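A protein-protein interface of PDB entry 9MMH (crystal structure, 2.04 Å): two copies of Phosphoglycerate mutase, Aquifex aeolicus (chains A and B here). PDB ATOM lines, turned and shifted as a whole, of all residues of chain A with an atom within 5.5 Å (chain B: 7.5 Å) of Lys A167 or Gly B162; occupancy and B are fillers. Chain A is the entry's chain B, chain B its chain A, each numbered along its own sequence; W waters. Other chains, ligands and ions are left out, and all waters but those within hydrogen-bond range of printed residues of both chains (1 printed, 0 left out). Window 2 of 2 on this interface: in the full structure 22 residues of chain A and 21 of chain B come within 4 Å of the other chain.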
ATOM      1  N   PRO A 111      -6.179  12.706  21.310  1.00  0.00           N
ATOM      2  CA  PRO A 111      -4.798  12.338  21.684  1.00  0.00           C
ATOM      3  C   PRO A 111      -4.307  13.084  22.891  1.00  0.00           C
ATOM      4  O   PRO A 111      -3.226  12.759  23.391  1.00  0.00           O
ATOM      5  CB  PRO A 111      -3.970  12.692  20.439  1.00  0.00           C
ATOM      6  CG  PRO A 111      -4.739  13.860  19.848  1.00  0.00           C
ATOM      7  CD  PRO A 111      -6.212  13.602  20.138  1.00  0.00           C
ATOM      8  N   CYS A 158      -5.311  23.229  14.361  1.00  0.00           N
ATOM      9  CA  CYS A 158      -6.165  23.183  15.535  1.00  0.00           C
ATOM     10  C   CYS A 158      -5.933  24.396  16.418  1.00  0.00           C
ATOM     11  O   CYS A 158      -6.894  25.000  16.909  1.00  0.00           O
ATOM     12  CB  CYS A 158      -5.928  21.887  16.313  1.00  0.00           C
ATOM     13  SG  CYS A 158      -6.532  20.411  15.479  1.00  0.00           S
ATOM     14  N   ILE A 163      -9.551  25.199  18.202  1.00  0.00           N
ATOM     15  CA  ILE A 163     -10.362  24.039  18.495  1.00  0.00           C
ATOM     16  C   ILE A 163      -9.642  23.001  19.351  1.00  0.00           C
ATOM     17  O   ILE A 163     -10.268  21.995  19.724  1.00  0.00           O
ATOM     18  CB  ILE A 163     -10.863  23.381  17.197  1.00  0.00           C
ATOM     19  CG1 ILE A 163      -9.688  23.025  16.287  1.00  0.00           C
ATOM     20  CG2 ILE A 163     -11.786  24.321  16.425  1.00  0.00           C
ATOM     21  CD1 ILE A 163     -10.090  22.257  15.072  1.00  0.00           C
ATOM     22  N   GLY A 164      -8.356  23.187  19.640  1.00  0.00           N
ATOM     23  CA  GLY A 164      -7.672  22.284  20.570  1.00  0.00           C
ATOM     24  C   GLY A 164      -7.081  21.063  19.888  1.00  0.00           C
ATOM     25  O   GLY A 164      -7.589  20.560  18.888  1.00  0.00           O
ATOM     26  N   LEU A 165      -5.970  20.565  20.448  1.00  0.00           N
ATOM     27  CA  LEU A 165      -5.321  19.405  19.861  1.00  0.00           C
ATOM     28  C   LEU A 165      -6.137  18.142  20.021  1.00  0.00           C
ATOM     29  O   LEU A 165      -5.811  17.129  19.387  1.00  0.00           O
ATOM     30  CB  LEU A 165      -3.938  19.202  20.470  1.00  0.00           C
ATOM     31  CG  LEU A 165      -2.888  20.272  20.190  1.00  0.00           C
ATOM     32  CD1 LEU A 165      -1.559  19.810  20.764  1.00  0.00           C
ATOM     33  CD2 LEU A 165      -2.731  20.554  18.728  1.00  0.00           C
ATOM     34  N   GLU A 166      -7.183  18.168  20.844  1.00  0.00           N
ATOM     35  CA  GLU A 166      -8.118  17.054  20.898  1.00  0.00           C
ATOM     36  C   GLU A 166      -8.610  16.678  19.499  1.00  0.00           C
ATOM     37  O   GLU A 166      -8.992  15.530  19.249  1.00  0.00           O
ATOM     38  CB  GLU A 166      -9.303  17.443  21.788  1.00  0.00           C
ATOM     39  CG  GLU A 166      -9.009  17.472  23.299  1.00  0.00           C
ATOM     40  CD  GLU A 166      -8.423  18.791  23.796  1.00  0.00           C
ATOM     41  OE1 GLU A 166      -8.259  19.734  23.000  1.00  0.00           O
ATOM     42  OE2 GLU A 166      -8.103  18.870  25.003  1.00  0.00           O
ATOM     43  N   LYS A 167      -8.604  17.631  18.578  1.00  0.00           N
ATOM     44  CA  LYS A 167      -9.184  17.445  17.254  1.00  0.00           C
ATOM     45  C   LYS A 167      -8.146  17.137  16.182  1.00  0.00           C
ATOM     46  O   LYS A 167      -8.503  17.044  15.001  1.00  0.00           O
ATOM     47  CB  LYS A 167      -9.969  18.706  16.874  1.00  0.00           C
ATOM     48  CG  LYS A 167     -11.158  19.009  17.817  1.00  0.00           C
ATOM     49  CD  LYS A 167     -12.163  17.846  17.885  1.00  0.00           C
ATOM     50  CE  LYS A 167     -13.329  18.118  18.847  1.00  0.00           C
ATOM     51  NZ  LYS A 167     -14.261  16.936  18.846  1.00  0.00           N
ATOM     52  N   MET A 168      -6.873  16.949  16.553  1.00  0.00           N
ATOM     53  CA  MET A 168      -5.841  16.967  15.523  1.00  0.00           C
ATOM     54  C   MET A 168      -5.927  15.778  14.575  1.00  0.00           C
ATOM     55  O   MET A 168      -5.371  15.841  13.476  1.00  0.00           O
ATOM     56  CB  MET A 168      -4.428  17.015  16.136  1.00  0.00           C
ATOM     57  CG  MET A 168      -4.026  15.865  17.071  1.00  0.00           C
ATOM     58  SD  MET A 168      -2.360  16.187  17.823  1.00  0.00           S
ATOM     59  CE  MET A 168      -1.289  16.217  16.447  1.00  0.00           C
ATOM     60  N   TRP A 169      -6.565  14.673  14.975  1.00  0.00           N
ATOM     61  CA  TRP A 169      -6.751  13.545  14.072  1.00  0.00           C
ATOM     62  C   TRP A 169      -8.195  13.436  13.568  1.00  0.00           C
ATOM     63  O   TRP A 169      -8.616  12.372  13.157  1.00  0.00           O
ATOM     64  CB  TRP A 169      -6.334  12.239  14.747  1.00  0.00           C
ATOM     65  CG  TRP A 169      -4.920  12.252  15.305  1.00  0.00           C
ATOM     66  CD1 TRP A 169      -4.554  11.985  16.603  1.00  0.00           C
ATOM     67  CD2 TRP A 169      -3.710  12.526  14.595  1.00  0.00           C
ATOM     68  NE1 TRP A 169      -3.189  12.104  16.745  1.00  0.00           N
ATOM     69  CE2 TRP A 169      -2.644  12.423  15.530  1.00  0.00           C
ATOM     70  CE3 TRP A 169      -3.416  12.863  13.271  1.00  0.00           C
ATOM     71  CZ2 TRP A 169      -1.322  12.620  15.177  1.00  0.00           C
ATOM     72  CZ3 TRP A 169      -2.096  13.078  12.919  1.00  0.00           C
ATOM     73  CH2 TRP A 169      -1.059  12.949  13.867  1.00  0.00           C
ATOM     74  N   HIS A 170      -8.950  14.513  13.618  1.00  0.00           N
ATOM     75  CA  HIS A 170     -10.252  14.622  12.974  1.00  0.00           C
ATOM     76  C   HIS A 170     -10.129  15.180  11.561  1.00  0.00           C
ATOM     77  O   HIS A 170     -11.149  15.399  10.898  1.00  0.00           O
ATOM     78  CB  HIS A 170     -11.140  15.556  13.789  1.00  0.00           C
ATOM     79  CG  HIS A 170     -11.792  14.921  14.979  1.00  0.00           C
ATOM     80  ND1 HIS A 170     -11.073  14.336  16.001  1.00  0.00           N
ATOM     81  CD2 HIS A 170     -13.100  14.776  15.308  1.00  0.00           C
ATOM     82  CE1 HIS A 170     -11.908  13.885  16.923  1.00  0.00           C
ATOM     83  NE2 HIS A 170     -13.143  14.122  16.519  1.00  0.00           N
ATOM     84  N   ILE A 171      -8.903  15.503  11.135  1.00  0.00           N
ATOM     85  CA  ILE A 171      -8.616  16.096   9.828  1.00  0.00           C
ATOM     86  C   ILE A 171      -7.487  15.301   9.205  1.00  0.00           C
ATOM     87  O   ILE A 171      -6.720  14.638   9.898  1.00  0.00           O
ATOM     88  CB  ILE A 171      -8.225  17.580   9.893  1.00  0.00           C
ATOM     89  CG1 ILE A 171      -6.930  17.735  10.688  1.00  0.00           C
ATOM     90  CG2 ILE A 171      -9.373  18.412  10.488  1.00  0.00           C
ATOM     91  CD1 ILE A 171      -6.506  19.152  10.827  1.00  0.00           C
ATOM     92  N   LEU B 156     -22.855  22.076   9.337  1.00  0.00           N
ATOM     93  CA  LEU B 156     -22.736  20.624   9.363  1.00  0.00           C
ATOM     94  C   LEU B 156     -21.303  20.172   9.701  1.00  0.00           C
ATOM     95  O   LEU B 156     -21.095  19.254  10.516  1.00  0.00           O
ATOM     96  CB  LEU B 156     -23.166  20.027   8.033  1.00  0.00           C
ATOM     97  CG  LEU B 156     -24.666  19.861   7.784  1.00  0.00           C
ATOM     98  CD1 LEU B 156     -24.836  19.534   6.271  1.00  0.00           C
ATOM     99  CD2 LEU B 156     -25.379  18.821   8.598  1.00  0.00           C
ATOM    100  N   LEU B 157     -20.308  20.760   9.042  1.00  0.00           N
ATOM    101  CA  LEU B 157     -18.917  20.384   9.331  1.00  0.00           C
ATOM    102  C   LEU B 157     -18.594  20.578  10.807  1.00  0.00           C
ATOM    103  O   LEU B 157     -18.008  19.702  11.451  1.00  0.00           O
ATOM    104  CB  LEU B 157     -17.943  21.214   8.503  1.00  0.00           C
ATOM    105  CG  LEU B 157     -17.623  20.675   7.140  1.00  0.00           C
ATOM    106  CD1 LEU B 157     -16.327  21.270   6.596  1.00  0.00           C
ATOM    107  CD2 LEU B 157     -17.551  19.155   7.162  1.00  0.00           C
ATOM    108  N   CYS B 158     -18.980  21.731  11.357  1.00  0.00           N
ATOM    109  CA  CYS B 158     -18.680  22.017  12.751  1.00  0.00           C
ATOM    110  C   CYS B 158     -19.326  20.993  13.673  1.00  0.00           C
ATOM    111  O   CYS B 158     -18.731  20.582  14.676  1.00  0.00           O
ATOM    112  CB  CYS B 158     -19.168  23.406  13.127  1.00  0.00           C
ATOM    113  SG  CYS B 158     -18.330  24.777  12.424  1.00  0.00           S
ATOM    114  N   LEU B 159     -20.563  20.594  13.377  1.00  0.00           N
ATOM    115  CA  LEU B 159     -21.227  19.650  14.267  1.00  0.00           C
ATOM    116  C   LEU B 159     -20.620  18.257  14.132  1.00  0.00           C
ATOM    117  O   LEU B 159     -20.425  17.550  15.121  1.00  0.00           O
ATOM    118  CB  LEU B 159     -22.728  19.609  13.969  1.00  0.00           C
ATOM    119  CG  LEU B 159     -23.531  20.885  14.239  1.00  0.00           C
ATOM    120  CD1 LEU B 159     -24.989  20.626  13.897  1.00  0.00           C
ATOM    121  CD2 LEU B 159     -23.340  21.347  15.673  1.00  0.00           C
ATOM    122  N   ALA B 160     -20.317  17.848  12.906  1.00  0.00           N
ATOM    123  CA  ALA B 160     -19.736  16.530  12.687  1.00  0.00           C
ATOM    124  C   ALA B 160     -18.407  16.381  13.417  1.00  0.00           C
ATOM    125  O   ALA B 160     -18.087  15.302  13.935  1.00  0.00           O
ATOM    126  CB  ALA B 160     -19.555  16.299  11.184  1.00  0.00           C
ATOM    127  N   LEU B 161     -17.603  17.439  13.438  1.00  0.00           N
ATOM    128  CA  LEU B 161     -16.314  17.409  14.107  1.00  0.00           C
ATOM    129  C   LEU B 161     -16.400  17.747  15.587  1.00  0.00           C
ATOM    130  O   LEU B 161     -15.383  17.695  16.274  1.00  0.00           O
ATOM    131  CB  LEU B 161     -15.360  18.395  13.435  1.00  0.00           C
ATOM    132  CG  LEU B 161     -15.131  18.016  11.956  1.00  0.00           C
ATOM    133  CD1 LEU B 161     -14.055  18.927  11.412  1.00  0.00           C
ATOM    134  CD2 LEU B 161     -14.760  16.581  11.729  1.00  0.00           C
ATOM    135  N   GLY B 162     -17.567  18.145  16.070  1.00  0.00           N
ATOM    136  CA  GLY B 162     -17.736  18.482  17.470  1.00  0.00           C
ATOM    137  C   GLY B 162     -17.075  19.756  17.908  1.00  0.00           C
ATOM    138  O   GLY B 162     -16.715  19.870  19.072  1.00  0.00           O
ATOM    139  N   ILE B 163     -16.906  20.729  17.014  1.00  0.00           N
ATOM    140  CA  ILE B 163     -16.215  21.963  17.379  1.00  0.00           C
ATOM    141  C   ILE B 163     -17.179  23.135  17.589  1.00  0.00           C
ATOM    142  O   ILE B 163     -16.730  24.237  17.894  1.00  0.00           O
ATOM    143  CB  ILE B 163     -15.148  22.356  16.337  1.00  0.00           C
ATOM    144  CG1 ILE B 163     -15.829  22.681  14.996  1.00  0.00           C
ATOM    145  CG2 ILE B 163     -14.126  21.249  16.118  1.00  0.00           C
ATOM    146  CD1 ILE B 163     -14.865  23.110  13.911  1.00  0.00           C
ATOM    147  N   GLY B 164     -18.468  22.953  17.360  1.00  0.00           N
ATOM    148  CA  GLY B 164     -19.400  24.013  17.757  1.00  0.00           C
ATOM    149  C   GLY B 164     -19.643  25.008  16.636  1.00  0.00           C
ATOM    150  O   GLY B 164     -18.761  25.361  15.854  1.00  0.00           O
ATOM    151  N   LEU B 165     -20.887  25.499  16.579  1.00  0.00           N
ATOM    152  CA  LEU B 165     -21.226  26.525  15.591  1.00  0.00           C
ATOM    153  C   LEU B 165     -20.502  27.852  15.824  1.00  0.00           C
ATOM    154  O   LEU B 165     -20.512  28.717  14.929  1.00  0.00           O
ATOM    155  CB  LEU B 165     -22.738  26.785  15.576  1.00  0.00           C
ATOM    156  CG  LEU B 165     -23.605  25.644  15.056  1.00  0.00           C
ATOM    157  CD1 LEU B 165     -25.055  26.089  14.865  1.00  0.00           C
ATOM    158  CD2 LEU B 165     -23.051  25.149  13.752  1.00  0.00           C
ATOM    159  N   ARG B 187     -17.939   8.138  14.258  1.00  0.00           N
ATOM    160  CA  ARG B 187     -17.414   9.493  14.280  1.00  0.00           C
ATOM    161  C   ARG B 187     -17.024   9.900  12.866  1.00  0.00           C
ATOM    162  O   ARG B 187     -17.022   9.093  11.938  1.00  0.00           O
ATOM    163  CB  ARG B 187     -16.218   9.594  15.227  1.00  0.00           C
ATOM    164  CG  ARG B 187     -15.124   8.604  14.854  1.00  0.00           C
ATOM    165  CD  ARG B 187     -13.788   9.074  15.389  1.00  0.00           C
ATOM    166  NE  ARG B 187     -13.329  10.271  14.687  1.00  0.00           N
ATOM    167  CZ  ARG B 187     -12.105  10.760  14.782  1.00  0.00           C
ATOM    168  NH1 ARG B 187     -11.182  10.170  15.537  1.00  0.00           N
ATOM    169  NH2 ARG B 187     -11.805  11.869  14.118  1.00  0.00           N
ATOM    170  N   PHE B 188     -16.702  11.170  12.721  1.00  0.00           N
ATOM    171  CA  PHE B 188     -16.404  11.776  11.433  1.00  0.00           C
ATOM    172  C   PHE B 188     -14.907  12.063  11.319  1.00  0.00           C
ATOM    173  O   PHE B 188     -14.193  12.156  12.323  1.00  0.00           O
ATOM    174  CB  PHE B 188     -17.221  13.062  11.271  1.00  0.00           C
ATOM    175  CG  PHE B 188     -18.717  12.843  11.119  1.00  0.00           C
ATOM    176  CD1 PHE B 188     -19.268  12.603   9.871  1.00  0.00           C
ATOM    177  CD2 PHE B 188     -19.567  12.938  12.210  1.00  0.00           C
ATOM    178  CE1 PHE B 188     -20.617  12.411   9.716  1.00  0.00           C
ATOM    179  CE2 PHE B 188     -20.935  12.752  12.058  1.00  0.00           C
ATOM    180  CZ  PHE B 188     -21.455  12.487  10.827  1.00  0.00           C
HETATM  181  O   HOH W   1     -15.796  17.688  21.082  1.00  0.00           O
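Among the printed residues, merely in contact across the chains: Lys A167 with Gly B162 (3.8 Å), His A170 with Leu B161 (3.8 Å) and Ile A163 with Ile B163 (3.9 Å).
The backbone carbonyl oxygen (O) of Trp A169 is in hydrogen-bond range of the guanidinium group (NH2) of Arg B187 (3.4 Å). The guanidinium group (NH2) of Arg B187 lies close to a ring nitrogen (ND1) of His A170. The backbone carbonyl oxygen of Leu B161 is in hydrogen-bond range of the side-chain amino group of Lys A167 (2.9 Å).
Hydrophobic or aromatic side chains of chain B within 4 Å of the printed part of chain A: Leu B161 and Ile B163. Along chain B the printed residues that touch a printed residue of chain A span positions 161 to 187.
N of Ile B163 sits at hydrogen-bond distance from O of Cys B158 (3.0 Å). O of Cys A158 sits at hydrogen-bond distance from N of Ile A163.
Ile A163 touches its own counterpart, Ile B163. 4 positions are printed for both chains.
Water W1 lies within hydrogen-bond range of NZ of Lys A167 (2.8 Å) and O of Gly B162 (3.1 Å).
Of the printed residues of chain B, Ile A163 touches Ile B163. Printed residues of chain B within 4 Å of Lys A167: Leu B161 (2.9 Å) and Gly B162 (3.8 Å). Of the printed residues of chain B, His A170 touches Leu B161 and Arg B187. Gly B162 touches just one residue of chain A: Lys A167. Of the printed residues of chain A, Ile B163 touches Ile A163 (3.9 Å). Printed residues of chain A within 4 Å of Arg B187: Trp A169 (3.4 Å) and His A170 (3.2 Å). The nearest printed residue of chain B that does not touch Trp A169 is Phe B188 (5.6 Å).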
